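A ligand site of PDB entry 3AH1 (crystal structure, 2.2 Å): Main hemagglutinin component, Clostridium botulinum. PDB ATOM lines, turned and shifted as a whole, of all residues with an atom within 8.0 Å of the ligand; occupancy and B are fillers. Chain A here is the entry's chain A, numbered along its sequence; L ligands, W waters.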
ATOM      1  N   PHE A 165      -0.117   6.977  33.395  1.00  0.00           N
ATOM      2  CA  PHE A 165      -0.669   5.705  32.938  1.00  0.00           C
ATOM      3  C   PHE A 165       0.399   4.643  32.814  1.00  0.00           C
ATOM      4  O   PHE A 165       1.575   4.946  32.605  1.00  0.00           O
ATOM      5  CB  PHE A 165      -1.354   5.884  31.583  1.00  0.00           C
ATOM      6  CG  PHE A 165      -2.602   6.726  31.629  1.00  0.00           C
ATOM      7  CD1 PHE A 165      -2.534   8.104  31.567  1.00  0.00           C
ATOM      8  CD2 PHE A 165      -3.849   6.128  31.731  1.00  0.00           C
ATOM      9  CE1 PHE A 165      -3.692   8.877  31.607  1.00  0.00           C
ATOM     10  CE2 PHE A 165      -5.007   6.888  31.775  1.00  0.00           C
ATOM     11  CZ  PHE A 165      -4.929   8.267  31.715  1.00  0.00           C
ATOM     12  N   LEU A 166      -0.033   3.394  32.910  1.00  0.00           N
ATOM     13  CA  LEU A 166       0.823   2.254  32.711  1.00  0.00           C
ATOM     14  C   LEU A 166       1.308   2.233  31.265  1.00  0.00           C
ATOM     15  O   LEU A 166       0.499   2.185  30.327  1.00  0.00           O
ATOM     16  CB  LEU A 166       0.054   0.963  33.044  1.00  0.00           C
ATOM     17  CG  LEU A 166       0.898  -0.289  33.203  1.00  0.00           C
ATOM     18  CD1 LEU A 166       1.732  -0.178  34.469  1.00  0.00           C
ATOM     19  CD2 LEU A 166       0.012  -1.531  33.240  1.00  0.00           C
ATOM     20  N   SER A 167       2.630   2.286  31.087  1.00  0.00           N
ATOM     21  CA  SER A 167       3.219   2.517  29.755  1.00  0.00           C
ATOM     22  C   SER A 167       4.497   1.742  29.554  1.00  0.00           C
ATOM     23  O   SER A 167       5.414   1.813  30.366  1.00  0.00           O
ATOM     24  CB  SER A 167       3.531   4.002  29.578  1.00  0.00           C
ATOM     25  OG  SER A 167       2.449   4.806  29.963  1.00  0.00           O
ATOM     26  N   LYS A 168       4.562   1.003  28.448  1.00  0.00           N
ATOM     27  CA  LYS A 168       5.820   0.478  27.962  1.00  0.00           C
ATOM     28  C   LYS A 168       6.677   1.671  27.570  1.00  0.00           C
ATOM     29  O   LYS A 168       6.182   2.606  26.942  1.00  0.00           O
ATOM     30  CB  LYS A 168       5.618  -0.396  26.735  1.00  0.00           C
ATOM     31  CG  LYS A 168       6.920  -0.918  26.131  1.00  0.00           C
ATOM     32  CD  LYS A 168       6.679  -1.654  24.822  1.00  0.00           C
ATOM     33  CE  LYS A 168       7.994  -2.024  24.133  1.00  0.00           C
ATOM     34  NZ  LYS A 168       8.803  -0.832  23.764  1.00  0.00           N
ATOM     35  N   ASN A 169       7.960   1.645  27.940  1.00  0.00           N
ATOM     36  CA  ASN A 169       8.859   2.745  27.610  1.00  0.00           C
ATOM     37  C   ASN A 169       9.340   2.642  26.162  1.00  0.00           C
ATOM     38  O   ASN A 169       9.348   1.557  25.597  1.00  0.00           O
ATOM     39  CB  ASN A 169      10.061   2.795  28.563  1.00  0.00           C
ATOM     40  CG  ASN A 169      10.404   4.212  28.981  1.00  0.00           C
ATOM     41  OD1 ASN A 169       9.599   5.126  28.847  1.00  0.00           O
ATOM     42  ND2 ASN A 169      11.611   4.403  29.520  1.00  0.00           N
ATOM     43  N   LEU A 170       9.742   3.766  25.593  1.00  0.00           N
ATOM     44  CA  LEU A 170      10.198   3.789  24.201  1.00  0.00           C
ATOM     45  C   LEU A 170      11.451   2.926  24.001  1.00  0.00           C
ATOM     46  O   LEU A 170      12.425   3.045  24.749  1.00  0.00           O
ATOM     47  CB  LEU A 170      10.473   5.222  23.735  1.00  0.00           C
ATOM     48  CG  LEU A 170      11.014   5.366  22.305  1.00  0.00           C
ATOM     49  CD1 LEU A 170      10.080   4.694  21.313  1.00  0.00           C
ATOM     50  CD2 LEU A 170      11.202   6.823  21.950  1.00  0.00           C
ATOM     51  N   ASN A 171      11.420   2.059  23.010  1.00  0.00           N
ATOM     52  CA  ASN A 171      12.591   1.266  22.642  1.00  0.00           C
ATOM     53  C   ASN A 171      13.236   0.603  23.868  1.00  0.00           C
ATOM     54  O   ASN A 171      14.471   0.571  24.011  1.00  0.00           O
ATOM     55  CB  ASN A 171      13.585   2.173  21.889  1.00  0.00           C
ATOM     56  CG  ASN A 171      14.412   1.417  20.866  1.00  0.00           C
ATOM     57  OD1 ASN A 171      13.889   0.681  20.021  1.00  0.00           O
ATOM     58  ND2 ASN A 171      15.729   1.616  20.914  1.00  0.00           N
ATOM     59  N   SER A 172      12.385   0.112  24.770  1.00  0.00           N
ATOM     60  CA  SER A 172      12.789  -0.731  25.903  1.00  0.00           C
ATOM     61  C   SER A 172      11.603  -1.604  26.333  1.00  0.00           C
ATOM     62  O   SER A 172      10.469  -1.322  25.959  1.00  0.00           O
ATOM     63  CB  SER A 172      13.250   0.119  27.073  1.00  0.00           C
ATOM     64  OG  SER A 172      13.536  -0.694  28.207  1.00  0.00           O
ATOM     65  N   ILE A 174      10.912  -2.165  29.615  1.00  0.00           N
ATOM     66  CA  ILE A 174      10.521  -1.728  30.950  1.00  0.00           C
ATOM     67  C   ILE A 174       9.207  -0.952  30.917  1.00  0.00           C
ATOM     68  O   ILE A 174       8.933  -0.233  29.944  1.00  0.00           O
ATOM     69  CB  ILE A 174      11.654  -0.901  31.607  1.00  0.00           C
ATOM     70  CG1 ILE A 174      12.863  -1.819  31.862  1.00  0.00           C
ATOM     71  CG2 ILE A 174      11.195  -0.280  32.914  1.00  0.00           C
ATOM     72  CD1 ILE A 174      14.161  -1.091  32.123  1.00  0.00           C
ATOM     73  N   ILE A 175       8.388  -1.148  31.952  1.00  0.00           N
ATOM     74  CA  ILE A 175       7.103  -0.484  32.099  1.00  0.00           C
ATOM     75  C   ILE A 175       7.243   0.626  33.117  1.00  0.00           C
ATOM     76  O   ILE A 175       7.775   0.420  34.217  1.00  0.00           O
ATOM     77  CB  ILE A 175       5.987  -1.455  32.570  1.00  0.00           C
ATOM     78  CG1 ILE A 175       5.870  -2.651  31.637  1.00  0.00           C
ATOM     79  CG2 ILE A 175       4.618  -0.751  32.671  1.00  0.00           C
ATOM     80  CD1 ILE A 175       5.722  -2.265  30.215  1.00  0.00           C
ATOM     81  N   VAL A 176       6.766   1.805  32.756  1.00  0.00           N
ATOM     82  CA  VAL A 176       6.880   2.982  33.594  1.00  0.00           C
ATOM     83  C   VAL A 176       5.552   3.736  33.617  1.00  0.00           C
ATOM     84  O   VAL A 176       4.635   3.426  32.865  1.00  0.00           O
ATOM     85  CB  VAL A 176       7.975   3.921  33.063  1.00  0.00           C
ATOM     86  CG1 VAL A 176       9.278   3.152  32.883  1.00  0.00           C
ATOM     87  CG2 VAL A 176       7.538   4.543  31.745  1.00  0.00           C
ATOM     88  N   LEU A 177       5.469   4.728  34.499  1.00  0.00           N
ATOM     89  CA  LEU A 177       4.417   5.702  34.446  1.00  0.00           C
ATOM     90  C   LEU A 177       4.712   6.682  33.316  1.00  0.00           C
ATOM     91  O   LEU A 177       5.868   7.069  33.115  1.00  0.00           O
ATOM     92  CB  LEU A 177       4.319   6.471  35.763  1.00  0.00           C
ATOM     93  CG  LEU A 177       3.699   5.757  36.969  1.00  0.00           C
ATOM     94  CD1 LEU A 177       3.669   6.707  38.149  1.00  0.00           C
ATOM     95  CD2 LEU A 177       2.289   5.286  36.631  1.00  0.00           C
ATOM     96  N   TRP A 178       3.667   7.087  32.598  1.00  0.00           N
ATOM     97  CA  TRP A 178       3.768   8.205  31.667  1.00  0.00           C
ATOM     98  C   TRP A 178       2.415   8.854  31.444  1.00  0.00           C
ATOM     99  O   TRP A 178       1.384   8.175  31.468  1.00  0.00           O
ATOM    100  CB  TRP A 178       4.349   7.771  30.322  1.00  0.00           C
ATOM    101  CG  TRP A 178       5.126   8.875  29.691  1.00  0.00           C
ATOM    102  CD1 TRP A 178       4.634   9.918  28.950  1.00  0.00           C
ATOM    103  CD2 TRP A 178       6.537   9.077  29.777  1.00  0.00           C
ATOM    104  NE1 TRP A 178       5.653  10.752  28.564  1.00  0.00           N
ATOM    105  CE2 TRP A 178       6.844  10.260  29.053  1.00  0.00           C
ATOM    106  CE3 TRP A 178       7.582   8.392  30.390  1.00  0.00           C
ATOM    107  CZ2 TRP A 178       8.134  10.758  28.939  1.00  0.00           C
ATOM    108  CZ3 TRP A 178       8.885   8.888  30.265  1.00  0.00           C
ATOM    109  CH2 TRP A 178       9.138  10.052  29.553  1.00  0.00           C
ATOM    110  N   GLN A 179       2.430  10.165  31.222  1.00  0.00           N
ATOM    111  CA  GLN A 179       1.214  10.893  30.865  1.00  0.00           C
ATOM    112  C   GLN A 179       0.643  10.371  29.553  1.00  0.00           C
ATOM    113  O   GLN A 179       1.372   9.802  28.745  1.00  0.00           O
ATOM    114  CB  GLN A 179       1.498  12.403  30.779  1.00  0.00           C
ATOM    115  CG  GLN A 179       2.375  12.807  29.595  1.00  0.00           C
ATOM    116  CD  GLN A 179       2.932  14.207  29.749  1.00  0.00           C
ATOM    117  OE1 GLN A 179       3.738  14.476  30.638  1.00  0.00           O
ATOM    118  NE2 GLN A 179       2.516  15.103  28.857  1.00  0.00           N
ATOM    119  N   TRP A 180      -0.666  10.541  29.379  1.00  0.00           N
ATOM    120  CA  TRP A 180      -1.346  10.032  28.190  1.00  0.00           C
ATOM    121  C   TRP A 180      -0.891  10.770  26.933  1.00  0.00           C
ATOM    122  O   TRP A 180      -0.953  11.993  26.890  1.00  0.00           O
ATOM    123  CB  TRP A 180      -2.864  10.208  28.371  1.00  0.00           C
ATOM    124  CG  TRP A 180      -3.698   9.610  27.305  1.00  0.00           C
ATOM    125  CD1 TRP A 180      -4.415  10.280  26.361  1.00  0.00           C
ATOM    126  CD2 TRP A 180      -3.917   8.220  27.063  1.00  0.00           C
ATOM    127  NE1 TRP A 180      -5.069   9.384  25.544  1.00  0.00           N
ATOM    128  CE2 TRP A 180      -4.787   8.110  25.955  1.00  0.00           C
ATOM    129  CE3 TRP A 180      -3.462   7.040  27.679  1.00  0.00           C
ATOM    130  CZ2 TRP A 180      -5.199   6.878  25.439  1.00  0.00           C
ATOM    131  CZ3 TRP A 180      -3.876   5.817  27.167  1.00  0.00           C
ATOM    132  CH2 TRP A 180      -4.736   5.748  26.050  1.00  0.00           C
ATOM    133  N   PHE A 181      -0.418  10.023  25.935  1.00  0.00           N
ATOM    134  CA  PHE A 181      -0.262  10.563  24.571  1.00  0.00           C
ATOM    135  C   PHE A 181      -0.805   9.582  23.506  1.00  0.00           C
ATOM    136  O   PHE A 181      -0.325   9.531  22.373  1.00  0.00           O
ATOM    137  CB  PHE A 181       1.198  10.983  24.287  1.00  0.00           C
ATOM    138  CG  PHE A 181       2.211   9.859  24.409  1.00  0.00           C
ATOM    139  CD1 PHE A 181       2.756   9.263  23.267  1.00  0.00           C
ATOM    140  CD2 PHE A 181       2.644   9.424  25.658  1.00  0.00           C
ATOM    141  CE1 PHE A 181       3.713   8.237  23.374  1.00  0.00           C
ATOM    142  CE2 PHE A 181       3.596   8.389  25.782  1.00  0.00           C
ATOM    143  CZ  PHE A 181       4.121   7.799  24.639  1.00  0.00           C
ATOM    144  N   SER A 183      -0.689   6.501  22.850  1.00  0.00           N
ATOM    145  CA  SER A 183       0.208   5.573  22.205  1.00  0.00           C
ATOM    146  C   SER A 183      -0.243   4.140  22.485  1.00  0.00           C
ATOM    147  O   SER A 183      -0.770   3.834  23.551  1.00  0.00           O
ATOM    148  CB  SER A 183       1.637   5.784  22.691  1.00  0.00           C
ATOM    149  OG  SER A 183       2.470   4.702  22.307  1.00  0.00           O
ATOM    150  N   ARG A 185       1.684   1.980  23.218  1.00  0.00           N
ATOM    151  CA  ARG A 185       2.492   1.607  24.382  1.00  0.00           C
ATOM    152  C   ARG A 185       1.741   1.734  25.708  1.00  0.00           C
ATOM    153  O   ARG A 185       2.190   1.187  26.717  1.00  0.00           O
ATOM    154  CB  ARG A 185       3.767   2.448  24.443  1.00  0.00           C
ATOM    155  CG  ARG A 185       4.722   2.129  23.328  1.00  0.00           C
ATOM    156  CD  ARG A 185       6.131   2.537  23.653  1.00  0.00           C
ATOM    157  NE  ARG A 185       6.312   3.988  23.720  1.00  0.00           N
ATOM    158  CZ  ARG A 185       6.404   4.782  22.656  1.00  0.00           C
ATOM    159  NH1 ARG A 185       6.288   4.301  21.420  1.00  0.00           N
ATOM    160  NH2 ARG A 185       6.597   6.086  22.829  1.00  0.00           N
ATOM    161  N   GLN A 186       0.631   2.473  25.704  1.00  0.00           N
ATOM    162  CA  GLN A 186      -0.198   2.698  26.877  1.00  0.00           C
ATOM    163  C   GLN A 186      -1.551   1.969  26.768  1.00  0.00           C
ATOM    164  O   GLN A 186      -2.490   2.270  27.510  1.00  0.00           O
ATOM    165  CB  GLN A 186      -0.428   4.217  27.049  1.00  0.00           C
ATOM    166  CG  GLN A 186       0.864   5.054  26.909  1.00  0.00           C
ATOM    167  CD  GLN A 186       0.625   6.535  26.975  1.00  0.00           C
ATOM    168  OE1 GLN A 186      -0.137   7.093  26.179  1.00  0.00           O
ATOM    169  NE2 GLN A 186       1.294   7.200  27.909  1.00  0.00           N
ATOM    170  N   GLU A 205       1.496  -2.200  21.605  1.00  0.00           N
ATOM    171  CA  GLU A 205       2.618  -1.760  20.787  1.00  0.00           C
ATOM    172  C   GLU A 205       3.448  -2.914  20.254  1.00  0.00           C
ATOM    173  O   GLU A 205       3.742  -2.948  19.073  1.00  0.00           O
ATOM    174  CB  GLU A 205       3.527  -0.800  21.574  1.00  0.00           C
ATOM    175  CG  GLU A 205       4.588  -0.099  20.717  1.00  0.00           C
ATOM    176  CD  GLU A 205       5.959  -0.711  20.836  1.00  0.00           C
ATOM    177  OE1 GLU A 205       6.705  -0.336  21.761  1.00  0.00           O
ATOM    178  OE2 GLU A 205       6.303  -1.569  19.990  1.00  0.00           O
ATOM    179  N   ASN A 266       6.993  11.275  35.021  1.00  0.00           N
ATOM    180  CA  ASN A 266       7.128  10.488  33.798  1.00  0.00           C
ATOM    181  C   ASN A 266       8.359   9.621  33.923  1.00  0.00           C
ATOM    182  O   ASN A 266       9.437  10.103  34.292  1.00  0.00           O
ATOM    183  CB  ASN A 266       7.280  11.410  32.563  1.00  0.00           C
ATOM    184  CG  ASN A 266       5.948  12.006  32.100  1.00  0.00           C
ATOM    185  OD1 ASN A 266       4.888  11.375  32.216  1.00  0.00           O
ATOM    186  ND2 ASN A 266       6.008  13.207  31.540  1.00  0.00           N
ATOM    187  N   GLY A 267       8.201   8.323  33.666  1.00  0.00           N
ATOM    188  CA  GLY A 267       9.324   7.404  33.710  1.00  0.00           C
ATOM    189  C   GLY A 267       9.530   6.672  35.026  1.00  0.00           C
ATOM    190  O   GLY A 267      10.365   5.768  35.091  1.00  0.00           O
HETATM  191  C1  LIG L   1      12.060  10.274  24.402  1.00  0.00           C
HETATM  192  C2  LIG L   1      11.026   9.861  25.447  1.00  0.00           C
HETATM  193  C3  LIG L   1      11.344   8.474  25.978  1.00  0.00           C
HETATM  194  C4  LIG L   1      10.143   7.894  26.742  1.00  0.00           C
HETATM  195  C5  LIG L   1       8.818   8.055  26.013  1.00  0.00           C
HETATM  196  C6  LIG L   1       8.624   9.524  25.643  1.00  0.00           C
HETATM  197  C7  LIG L   1       7.317   9.746  24.872  1.00  0.00           C
HETATM  198  C8  LIG L   1       7.093  11.204  24.465  1.00  0.00           C
HETATM  199  C9  LIG L   1       5.891  11.351  23.533  1.00  0.00           C
HETATM  200  C10 LIG L   1       7.082   6.514  26.721  1.00  0.00           C
HETATM  201  C11 LIG L   1       6.053   6.187  27.758  1.00  0.00           C
HETATM  202  N1  LIG L   1       7.776   7.632  26.943  1.00  0.00           N
HETATM  203  O1  LIG L   1      11.670  10.611  23.248  1.00  0.00           O
HETATM  204  O2  LIG L   1      13.272  10.287  24.755  1.00  0.00           O
HETATM  205  O3  LIG L   1      11.043  10.800  26.537  1.00  0.00           O
HETATM  206  O4  LIG L   1      10.330   6.497  26.974  1.00  0.00           O
HETATM  207  O5  LIG L   1       9.743   9.882  24.824  1.00  0.00           O
HETATM  208  O6  LIG L   1       7.301   8.912  23.714  1.00  0.00           O
HETATM  209  O7  LIG L   1       6.871  12.017  25.623  1.00  0.00           O
HETATM  210  O8  LIG L   1       5.296  12.649  23.723  1.00  0.00           O
HETATM  211  O9  LIG L   1       7.253   5.784  25.753  1.00  0.00           O
HETATM  212  O   HOH W   1       5.782   9.140  20.725  1.00  0.00           O
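The side-chain amide oxygen of Asn 169 sits at hydrogen-bond distance from an oxygen (O4) of the ligand, at 2.4 Å. An oxygen (O9) of the ligand lies within hydrogen-bond range of the guanidinium group (NE) of Arg 185. O4 of the ligand sits at hydrogen-bond distance from N of Leu 170. An oxygen (O7) of the ligand is in hydrogen-bond range of the indole nitrogen of Trp 178.
The backbone NH (N) of Asn 169 lies within hydrogen-bond range of the backbone carbonyl oxygen (O) of Ile 174 (2.9 Å). O of Trp 178 sits at hydrogen-bond distance from N of Phe 165 (2.7 Å). The backbone NH (N) of Phe 181 is in hydrogen-bond range of the side-chain amide oxygen (OE1) of Gln 186, 3.0 Å away. The side-chain amino group (NZ) of Lys 168 is in hydrogen-bond range of the backbone carbonyl oxygen (O) of Ser 172, at 2.8 Å. NZ of Lys 168 lies within salt-bridge range of OE1 of Glu 205 (2.9 Å). N of Val 176 is in hydrogen-bond range of O of Ser 167 (2.7 Å). The side-chain hydroxyl (OG) of Ser 167 sits at hydrogen-bond distance from the side-chain amide nitrogen (NE2) of Gln 186 (3.4 Å). The side-chain hydroxyl (OG) of Ser 167 is in hydrogen-bond range of the backbone carbonyl oxygen (O) of Phe 165, at 2.8 Å.
Merely in contact with the ligand: Phe 181 (3.5 Å), Lys 168 (3.6 Å) and Ser 167 (3.8 Å). Hydrophobic or aromatic side chains that line the ligand: Leu 170, Trp 178 and Phe 181. Within 4 Å of the ligand: Ser 167, Lys 168, Asn 169, Leu 170, Trp 178, Phe 181 and Arg 185.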
